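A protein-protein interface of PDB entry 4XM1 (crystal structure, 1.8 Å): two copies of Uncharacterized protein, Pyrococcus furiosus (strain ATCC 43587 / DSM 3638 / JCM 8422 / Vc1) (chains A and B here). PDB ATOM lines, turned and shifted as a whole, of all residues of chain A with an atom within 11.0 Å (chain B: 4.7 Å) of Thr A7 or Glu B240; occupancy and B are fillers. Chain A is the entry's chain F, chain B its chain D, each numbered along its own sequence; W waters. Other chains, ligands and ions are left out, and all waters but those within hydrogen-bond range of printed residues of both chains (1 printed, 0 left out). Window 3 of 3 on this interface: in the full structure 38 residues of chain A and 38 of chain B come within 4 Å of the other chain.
N of Phe A8 is in hydrogen-bond range of OE2 of Glu B240 (2.9 Å).
Water W1 lies within hydrogen-bond range of the side-chain carboxylate (OE1) of Glu B240 (2.5 Å), the backbone NH (N) of Glu A9 (2.8 Å) and the backbone NH (N) of Phe A8 (3.5 Å).
N of Ser A6 lies within hydrogen-bond range of OE1 of Glu A10, at 2.9 Å. The side-chain hydroxyl of Thr A7 lies within hydrogen-bond range of the backbone NH of Glu A10.
Hydrophobic or aromatic side chains of chain A within 4 Å of the printed part of chain B: Val A5, Phe A8 and Ala A11. Of the 9 printed residues of chain B, 3 touch a printed residue of chain A. Among the printed residues, 8 pairs touch across the chains. Among the printed residues, no Asp or Glu carboxylate lies within 4 Å of a Lys or Arg side-chain nitrogen of the other chain.
Among the printed residues, pairs that only touch across the chains: Val A5 with Met B236 (3.9 Å), Ser A6 with Met B236 (3.9 Å), Thr A7 with Met B236 (3.4 Å), Thr A7 with Glu B240 (3.4 Å), Phe A8 with Met B236 (3.9 Å), Phe A8 with Phe B237 (3.6 Å) and Ala A11 with Met B236 (3.8 Å).
No position is printed for both chains. Of the 8 pairs that touch across the chains among the printed residues, none has its exchanged pair printed and touching as well.
Thr A7 touches just these residues of chain B: Met B236 (3.4 Å) and Glu B240 (3.4 Å). Of chain A, only Val A5, Ser A6, Thr A7, Phe A8 and Ala A11 come within 4 Å of Met B236. No residue of chain A comes within 4 Å of Gly B239. No residue of chain A comes within 4 Å of Ile B242. No residue of chain A comes within 4 Å of Gly B243. Of the printed residues of chain A, Phe B237 touches Phe A8 (3.6 Å). Of the printed residues of chain B, Val A5 touches Met B236 (3.9 Å). Of the printed residues of chain B, Ser A6 touches Met B236 (3.9 Å). Of the printed residues of chain B, Phe A8 touches Met B236 (3.9 Å), Phe B237 (3.6 Å) and Glu B240 (2.9 Å). Printed residues of chain B within 4 Å of Ala A11: Met B236. The nearest printed residue of chain B that does not touch Val A5 is Glu B240 (8.3 Å).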
ATOM      1  N   PHE A   2     -31.411 -30.506  -7.854  1.00  0.00           N
ATOM      2  CA  PHE A   2     -30.126 -29.804  -7.838  1.00  0.00           C
ATOM      3  C   PHE A   2     -29.412 -29.929  -9.163  1.00  0.00           C
ATOM      4  O   PHE A   2     -28.176 -29.906  -9.221  1.00  0.00           O
ATOM      5  CB  PHE A   2     -29.234 -30.348  -6.697  1.00  0.00           C
ATOM      6  CG  PHE A   2     -29.281 -29.522  -5.471  1.00  0.00           C
ATOM      7  CD1 PHE A   2     -28.117 -29.046  -4.882  1.00  0.00           C
ATOM      8  CD2 PHE A   2     -30.503 -29.121  -4.945  1.00  0.00           C
ATOM      9  CE1 PHE A   2     -28.189 -28.255  -3.743  1.00  0.00           C
ATOM     10  CE2 PHE A   2     -30.585 -28.342  -3.835  1.00  0.00           C
ATOM     11  CZ  PHE A   2     -29.437 -27.897  -3.211  1.00  0.00           C
ATOM     12  N   GLU A   3     -30.187 -30.055 -10.227  1.00  0.00           N
ATOM     13  CA  GLU A   3     -29.642 -30.231 -11.553  1.00  0.00           C
ATOM     14  C   GLU A   3     -29.462 -28.899 -12.263  1.00  0.00           C
ATOM     15  O   GLU A   3     -28.758 -28.847 -13.215  1.00  0.00           O
ATOM     16  CB  GLU A   3     -30.544 -31.154 -12.374  1.00  0.00           C
ATOM     17  CG  GLU A   3     -30.128 -32.633 -12.268  1.00  0.00           C
ATOM     18  CD  GLU A   3     -31.273 -33.565 -12.410  1.00  0.00           C
ATOM     19  OE1 GLU A   3     -32.305 -33.315 -11.749  1.00  0.00           O
ATOM     20  OE2 GLU A   3     -31.155 -34.550 -13.171  1.00  0.00           O
ATOM     21  N   ASN A   4     -30.119 -27.844 -11.804  1.00  0.00           N
ATOM     22  CA  ASN A   4     -30.046 -26.541 -12.471  1.00  0.00           C
ATOM     23  C   ASN A   4     -29.136 -25.536 -11.778  1.00  0.00           C
ATOM     24  O   ASN A   4     -29.026 -24.371 -12.202  1.00  0.00           O
ATOM     25  CB  ASN A   4     -31.439 -25.940 -12.666  1.00  0.00           C
ATOM     26  CG  ASN A   4     -32.334 -26.787 -13.581  1.00  0.00           C
ATOM     27  OD1 ASN A   4     -31.950 -27.853 -14.049  1.00  0.00           O
ATOM     28  ND2 ASN A   4     -33.536 -26.307 -13.825  1.00  0.00           N
ATOM     29  N   VAL A   5     -28.488 -25.945 -10.698  1.00  0.00           N
ATOM     30  CA  VAL A   5     -27.360 -25.119 -10.208  1.00  0.00           C
ATOM     31  C   VAL A   5     -26.155 -25.271 -11.170  1.00  0.00           C
ATOM     32  O   VAL A   5     -25.962 -26.308 -11.815  1.00  0.00           O
ATOM     33  CB  VAL A   5     -27.021 -25.383  -8.701  1.00  0.00           C
ATOM     34  CG1 VAL A   5     -28.212 -24.931  -7.803  1.00  0.00           C
ATOM     35  CG2 VAL A   5     -26.735 -26.858  -8.483  1.00  0.00           C
ATOM     36  N   SER A   6     -25.340 -24.226 -11.256  1.00  0.00           N
ATOM     37  CA  SER A   6     -24.277 -24.151 -12.233  1.00  0.00           C
ATOM     38  C   SER A   6     -22.844 -24.230 -11.702  1.00  0.00           C
ATOM     39  O   SER A   6     -21.923 -24.577 -12.457  1.00  0.00           O
ATOM     40  CB  SER A   6     -24.385 -22.823 -13.008  1.00  0.00           C
ATOM     41  OG  SER A   6     -25.259 -22.987 -14.105  1.00  0.00           O
ATOM     42  N   THR A   7     -22.648 -23.807 -10.454  1.00  0.00           N
ATOM     43  CA  THR A   7     -21.342 -23.842  -9.828  1.00  0.00           C
ATOM     44  C   THR A   7     -21.471 -24.412  -8.427  1.00  0.00           C
ATOM     45  O   THR A   7     -22.566 -24.404  -7.867  1.00  0.00           O
ATOM     46  CB  THR A   7     -20.788 -22.461  -9.614  1.00  0.00           C
ATOM     47  OG1 THR A   7     -21.685 -21.724  -8.772  1.00  0.00           O
ATOM     48  CG2 THR A   7     -20.557 -21.734 -10.990  1.00  0.00           C
ATOM     49  N   PHE A   8     -20.339 -24.842  -7.863  1.00  0.00           N
ATOM     50  CA  PHE A   8     -20.328 -25.300  -6.500  1.00  0.00           C
ATOM     51  C   PHE A   8     -20.843 -24.250  -5.509  1.00  0.00           C
ATOM     52  O   PHE A   8     -21.628 -24.583  -4.622  1.00  0.00           O
ATOM     53  CB  PHE A   8     -18.948 -25.787  -6.070  1.00  0.00           C
ATOM     54  CG  PHE A   8     -18.824 -25.921  -4.585  1.00  0.00           C
ATOM     55  CD1 PHE A   8     -19.484 -26.956  -3.920  1.00  0.00           C
ATOM     56  CD2 PHE A   8     -18.142 -24.947  -3.846  1.00  0.00           C
ATOM     57  CE1 PHE A   8     -19.398 -27.058  -2.545  1.00  0.00           C
ATOM     58  CE2 PHE A   8     -18.050 -25.028  -2.479  1.00  0.00           C
ATOM     59  CZ  PHE A   8     -18.697 -26.091  -1.811  1.00  0.00           C
ATOM     60  N   GLU A   9     -20.405 -22.999  -5.657  1.00  0.00           N
ATOM     61  CA  GLU A   9     -20.862 -21.959  -4.763  1.00  0.00           C
ATOM     62  C   GLU A   9     -22.401 -21.839  -4.772  1.00  0.00           C
ATOM     63  O   GLU A   9     -23.013 -21.698  -3.734  1.00  0.00           O
ATOM     64  CB  GLU A   9     -20.208 -20.602  -5.094  1.00  0.00           C
ATOM     65  CG  GLU A   9     -20.518 -19.548  -4.021  1.00  0.00           C
ATOM     66  CD  GLU A   9     -19.895 -18.196  -4.314  1.00  0.00           C
ATOM     67  OE1 GLU A   9     -19.130 -17.710  -3.459  1.00  0.00           O
ATOM     68  OE2 GLU A   9     -20.175 -17.618  -5.388  1.00  0.00           O
ATOM     69  N   GLU A  10     -22.999 -21.886  -5.951  1.00  0.00           N
ATOM     70  CA  GLU A  10     -24.447 -21.835  -6.058  1.00  0.00           C
ATOM     71  C   GLU A  10     -25.052 -23.028  -5.331  1.00  0.00           C
ATOM     72  O   GLU A  10     -26.010 -22.866  -4.545  1.00  0.00           O
ATOM     73  CB  GLU A  10     -24.894 -21.829  -7.513  1.00  0.00           C
ATOM     74  CG  GLU A  10     -26.333 -21.348  -7.706  1.00  0.00           C
ATOM     75  CD  GLU A  10     -26.828 -21.404  -9.171  1.00  0.00           C
ATOM     76  OE1 GLU A  10     -26.016 -21.689 -10.092  1.00  0.00           O
ATOM     77  OE2 GLU A  10     -28.041 -21.141  -9.393  1.00  0.00           O
ATOM     78  N   ALA A  11     -24.504 -24.213  -5.582  1.00  0.00           N
ATOM     79  CA  ALA A  11     -25.009 -25.438  -4.939  1.00  0.00           C
ATOM     80  C   ALA A  11     -24.911 -25.367  -3.380  1.00  0.00           C
ATOM     81  O   ALA A  11     -25.846 -25.696  -2.691  1.00  0.00           O
ATOM     82  CB  ALA A  11     -24.266 -26.653  -5.498  1.00  0.00           C
ATOM     83  N   PHE A  12     -23.792 -24.902  -2.855  1.00  0.00           N
ATOM     84  CA  PHE A  12     -23.528 -24.818  -1.429  1.00  0.00           C
ATOM     85  C   PHE A  12     -24.511 -23.848  -0.765  1.00  0.00           C
ATOM     86  O   PHE A  12     -25.141 -24.196   0.224  1.00  0.00           O
ATOM     87  CB  PHE A  12     -22.041 -24.404  -1.223  1.00  0.00           C
ATOM     88  CG  PHE A  12     -21.660 -24.128   0.201  1.00  0.00           C
ATOM     89  CD1 PHE A  12     -21.161 -25.146   1.028  1.00  0.00           C
ATOM     90  CD2 PHE A  12     -21.770 -22.851   0.711  1.00  0.00           C
ATOM     91  CE1 PHE A  12     -20.773 -24.878   2.365  1.00  0.00           C
ATOM     92  CE2 PHE A  12     -21.384 -22.560   2.055  1.00  0.00           C
ATOM     93  CZ  PHE A  12     -20.872 -23.565   2.875  1.00  0.00           C
ATOM     94  N   ASN A  13     -24.654 -22.643  -1.316  1.00  0.00           N
ATOM     95  CA  ASN A  13     -25.677 -21.678  -0.847  1.00  0.00           C
ATOM     96  C   ASN A  13     -27.080 -22.251  -0.763  1.00  0.00           C
ATOM     97  O   ASN A  13     -27.789 -22.053   0.251  1.00  0.00           O
ATOM     98  CB  ASN A  13     -25.700 -20.455  -1.742  1.00  0.00           C
ATOM     99  CG  ASN A  13     -24.541 -19.516  -1.462  1.00  0.00           C
ATOM    100  OD1 ASN A  13     -23.955 -19.514  -0.374  1.00  0.00           O
ATOM    101  ND2 ASN A  13     -24.220 -18.692  -2.437  1.00  0.00           N
ATOM    102  N   LYS A  14     -27.478 -22.953  -1.820  1.00  0.00           N
ATOM    103  CA  LYS A  14     -28.822 -23.548  -1.872  1.00  0.00           C
ATOM    104  C   LYS A  14     -28.975 -24.694  -0.865  1.00  0.00           C
ATOM    105  O   LYS A  14     -30.010 -24.822  -0.206  1.00  0.00           O
ATOM    106  CB  LYS A  14     -29.153 -24.009  -3.283  1.00  0.00           C
ATOM    107  CG  LYS A  14     -30.611 -24.562  -3.509  1.00  0.00           C
ATOM    108  CD  LYS A  14     -30.764 -25.044  -4.962  1.00  0.00           C
ATOM    109  CE  LYS A  14     -32.176 -25.577  -5.315  1.00  0.00           C
ATOM    110  NZ  LYS A  14     -33.154 -24.431  -5.391  1.00  0.00           N
ATOM    111  N   LEU A  15     -27.943 -25.523  -0.772  1.00  0.00           N
ATOM    112  CA  LEU A  15     -27.932 -26.632   0.175  1.00  0.00           C
ATOM    113  C   LEU A  15     -28.083 -26.053   1.585  1.00  0.00           C
ATOM    114  O   LEU A  15     -28.942 -26.498   2.355  1.00  0.00           O
ATOM    115  CB  LEU A  15     -26.640 -27.457   0.000  1.00  0.00           C
ATOM    116  CG  LEU A  15     -26.453 -28.578   1.023  1.00  0.00           C
ATOM    117  CD1 LEU A  15     -27.549 -29.639   0.873  1.00  0.00           C
ATOM    118  CD2 LEU A  15     -25.090 -29.207   0.916  1.00  0.00           C
ATOM    119  N   LEU A  16     -27.293 -25.022   1.920  1.00  0.00           N
ATOM    120  CA  LEU A  16     -27.436 -24.421   3.254  1.00  0.00           C
ATOM    121  C   LEU A  16     -28.836 -23.814   3.497  1.00  0.00           C
ATOM    122  O   LEU A  16     -29.519 -24.161   4.508  1.00  0.00           O
ATOM    123  CB  LEU A  16     -26.355 -23.334   3.510  1.00  0.00           C
ATOM    124  CG  LEU A  16     -24.985 -23.745   4.108  1.00  0.00           C
ATOM    125  CD1 LEU A  16     -24.135 -22.519   4.342  1.00  0.00           C
ATOM    126  CD2 LEU A  16     -25.107 -24.527   5.420  1.00  0.00           C
ATOM    127  N   PHE A 263     -16.549 -29.733   2.736  1.00  0.00           N
ATOM    128  CA  PHE A 263     -16.715 -28.286   2.762  1.00  0.00           C
ATOM    129  C   PHE A 263     -17.257 -27.785   4.131  1.00  0.00           C
ATOM    130  O   PHE A 263     -17.726 -26.628   4.275  1.00  0.00           O
ATOM    131  CB  PHE A 263     -17.517 -27.772   1.513  1.00  0.00           C
ATOM    132  CG  PHE A 263     -18.824 -28.512   1.251  1.00  0.00           C
ATOM    133  CD1 PHE A 263     -18.931 -29.376   0.174  1.00  0.00           C
ATOM    134  CD2 PHE A 263     -19.948 -28.302   2.082  1.00  0.00           C
ATOM    135  CE1 PHE A 263     -20.145 -30.095  -0.055  1.00  0.00           C
ATOM    136  CE2 PHE A 263     -21.168 -29.000   1.862  1.00  0.00           C
ATOM    137  CZ  PHE A 263     -21.259 -29.901   0.809  1.00  0.00           C
ATOM    138  N   LEU A 266     -16.303 -24.432   5.486  1.00  0.00           N
ATOM    139  CA  LEU A 266     -16.727 -23.239   4.738  1.00  0.00           C
ATOM    140  C   LEU A 266     -17.707 -22.399   5.519  1.00  0.00           C
ATOM    141  O   LEU A 266     -17.962 -21.259   5.164  1.00  0.00           O
ATOM    142  CB  LEU A 266     -17.185 -23.525   3.278  1.00  0.00           C
ATOM    143  CG  LEU A 266     -16.032 -23.907   2.307  1.00  0.00           C
ATOM    144  CD1 LEU A 266     -16.459 -24.047   0.878  1.00  0.00           C
ATOM    145  CD2 LEU A 266     -14.784 -22.949   2.401  1.00  0.00           C
ATOM    146  N   MET B 236     -19.835 -31.738  -7.092  1.00  0.00           N
ATOM    147  CA  MET B 236     -19.577 -30.431  -7.731  1.00  0.00           C
ATOM    148  C   MET B 236     -18.383 -29.758  -7.100  1.00  0.00           C
ATOM    149  O   MET B 236     -17.576 -29.119  -7.798  1.00  0.00           O
ATOM    150  CB  MET B 236     -20.816 -29.506  -7.646  1.00  0.00           C
ATOM    151  CG  MET B 236     -21.919 -29.869  -8.609  1.00  0.00           C
ATOM    152  SD  MET B 236     -23.387 -28.794  -8.528  1.00  0.00           S
ATOM    153  CE  MET B 236     -22.769 -27.412  -9.511  1.00  0.00           C
ATOM    154  N   PHE B 237     -18.275 -29.871  -5.775  1.00  0.00           N
ATOM    155  CA  PHE B 237     -17.058 -29.382  -5.052  1.00  0.00           C
ATOM    156  C   PHE B 237     -15.727 -29.907  -5.678  1.00  0.00           C
ATOM    157  O   PHE B 237     -14.768 -29.150  -5.843  1.00  0.00           O
ATOM    158  CB  PHE B 237     -17.195 -29.784  -3.565  1.00  0.00           C
ATOM    159  CG  PHE B 237     -15.977 -29.551  -2.746  1.00  0.00           C
ATOM    160  CD1 PHE B 237     -15.107 -30.616  -2.444  1.00  0.00           C
ATOM    161  CD2 PHE B 237     -15.622 -28.273  -2.360  1.00  0.00           C
ATOM    162  CE1 PHE B 237     -13.948 -30.426  -1.691  1.00  0.00           C
ATOM    163  CE2 PHE B 237     -14.453 -28.059  -1.608  1.00  0.00           C
ATOM    164  CZ  PHE B 237     -13.628 -29.131  -1.250  1.00  0.00           C
ATOM    165  N   TYR B 238     -15.700 -31.197  -5.976  1.00  0.00           N
ATOM    166  CA  TYR B 238     -14.542 -31.887  -6.552  1.00  0.00           C
ATOM    167  C   TYR B 238     -14.416 -31.570  -8.046  1.00  0.00           C
ATOM    168  O   TYR B 238     -13.387 -31.040  -8.487  1.00  0.00           O
ATOM    169  CB  TYR B 238     -14.643 -33.397  -6.348  1.00  0.00           C
ATOM    170  CG  TYR B 238     -14.567 -33.880  -4.896  1.00  0.00           C
ATOM    171  CD1 TYR B 238     -13.501 -33.515  -4.062  1.00  0.00           C
ATOM    172  CD2 TYR B 238     -15.552 -34.723  -4.372  1.00  0.00           C
ATOM    173  CE1 TYR B 238     -13.410 -33.983  -2.737  1.00  0.00           C
ATOM    174  CE2 TYR B 238     -15.487 -35.189  -3.054  1.00  0.00           C
ATOM    175  CZ  TYR B 238     -14.410 -34.838  -2.243  1.00  0.00           C
ATOM    176  OH  TYR B 238     -14.296 -35.259  -0.931  1.00  0.00           O
ATOM    177  N   GLY B 239     -15.473 -31.864  -8.803  1.00  0.00           N
ATOM    178  CA  GLY B 239     -15.531 -31.599 -10.249  1.00  0.00           C
ATOM    179  C   GLY B 239     -14.967 -30.215 -10.583  1.00  0.00           C
ATOM    180  O   GLY B 239     -14.100 -30.067 -11.457  1.00  0.00           O
ATOM    181  N   GLU B 240     -15.427 -29.191  -9.864  1.00  0.00           N
ATOM    182  CA  GLU B 240     -15.044 -27.821 -10.173  1.00  0.00           C
ATOM    183  C   GLU B 240     -13.561 -27.576 -10.077  1.00  0.00           C
ATOM    184  O   GLU B 240     -13.033 -26.660 -10.747  1.00  0.00           O
ATOM    185  CB  GLU B 240     -15.762 -26.863  -9.231  1.00  0.00           C
ATOM    186  CG  GLU B 240     -15.744 -25.445  -9.686  1.00  0.00           C
ATOM    187  CD  GLU B 240     -16.877 -24.641  -9.110  1.00  0.00           C
ATOM    188  OE1 GLU B 240     -16.568 -23.856  -8.197  1.00  0.00           O
ATOM    189  OE2 GLU B 240     -18.040 -24.802  -9.574  1.00  0.00           O
ATOM    190  N   LYS B 241     -12.875 -28.361  -9.251  1.00  0.00           N
ATOM    191  CA  LYS B 241     -11.407 -28.241  -9.123  1.00  0.00           C
ATOM    192  C   LYS B 241     -10.615 -28.529 -10.430  1.00  0.00           C
ATOM    193  O   LYS B 241      -9.478 -28.074 -10.601  1.00  0.00           O
ATOM    194  CB  LYS B 241     -10.912 -29.145  -7.991  1.00  0.00           C
ATOM    195  CG  LYS B 241     -11.233 -28.568  -6.603  1.00  0.00           C
ATOM    196  CD  LYS B 241     -10.846 -29.519  -5.486  1.00  0.00           C
ATOM    197  CE  LYS B 241     -11.423 -29.075  -4.156  1.00  0.00           C
ATOM    198  NZ  LYS B 241     -11.348 -27.604  -3.926  1.00  0.00           N
ATOM    199  N   ILE B 242     -11.214 -29.307 -11.320  1.00  0.00           N
ATOM    200  CA  ILE B 242     -10.598 -29.631 -12.631  1.00  0.00           C
ATOM    201  C   ILE B 242     -11.559 -29.266 -13.778  1.00  0.00           C
ATOM    202  O   ILE B 242     -11.490 -29.816 -14.875  1.00  0.00           O
ATOM    203  CB  ILE B 242     -10.133 -31.081 -12.717  1.00  0.00           C
ATOM    204  CG1 ILE B 242     -11.294 -32.033 -12.427  1.00  0.00           C
ATOM    205  CG2 ILE B 242      -8.992 -31.319 -11.691  1.00  0.00           C
ATOM    206  CD1 ILE B 242     -11.284 -33.272 -13.227  1.00  0.00           C
ATOM    207  N   GLY B 243     -12.482 -28.362 -13.484  1.00  0.00           N
ATOM    208  CA  GLY B 243     -13.342 -27.777 -14.486  1.00  0.00           C
ATOM    209  C   GLY B 243     -14.311 -28.730 -15.125  1.00  0.00           C
ATOM    210  O   GLY B 243     -14.637 -28.579 -16.301  1.00  0.00           O
ATOM    211  N   VAL B 244     -14.789 -29.715 -14.369  1.00  0.00           N
ATOM    212  CA  VAL B 244     -15.851 -30.599 -14.853  1.00  0.00           C
ATOM    213  C   VAL B 244     -17.115 -30.435 -13.943  1.00  0.00           C
ATOM    214  O   VAL B 244     -17.025 -29.849 -12.861  1.00  0.00           O
ATOM    215  CB  VAL B 244     -15.379 -32.088 -14.957  1.00  0.00           C
ATOM    216  CG1 VAL B 244     -14.304 -32.303 -16.043  1.00  0.00           C
ATOM    217  CG2 VAL B 244     -14.883 -32.624 -13.587  1.00  0.00           C
HETATM  218  O   HOH W   1     -18.150 -22.255  -7.114  1.00  0.00           O
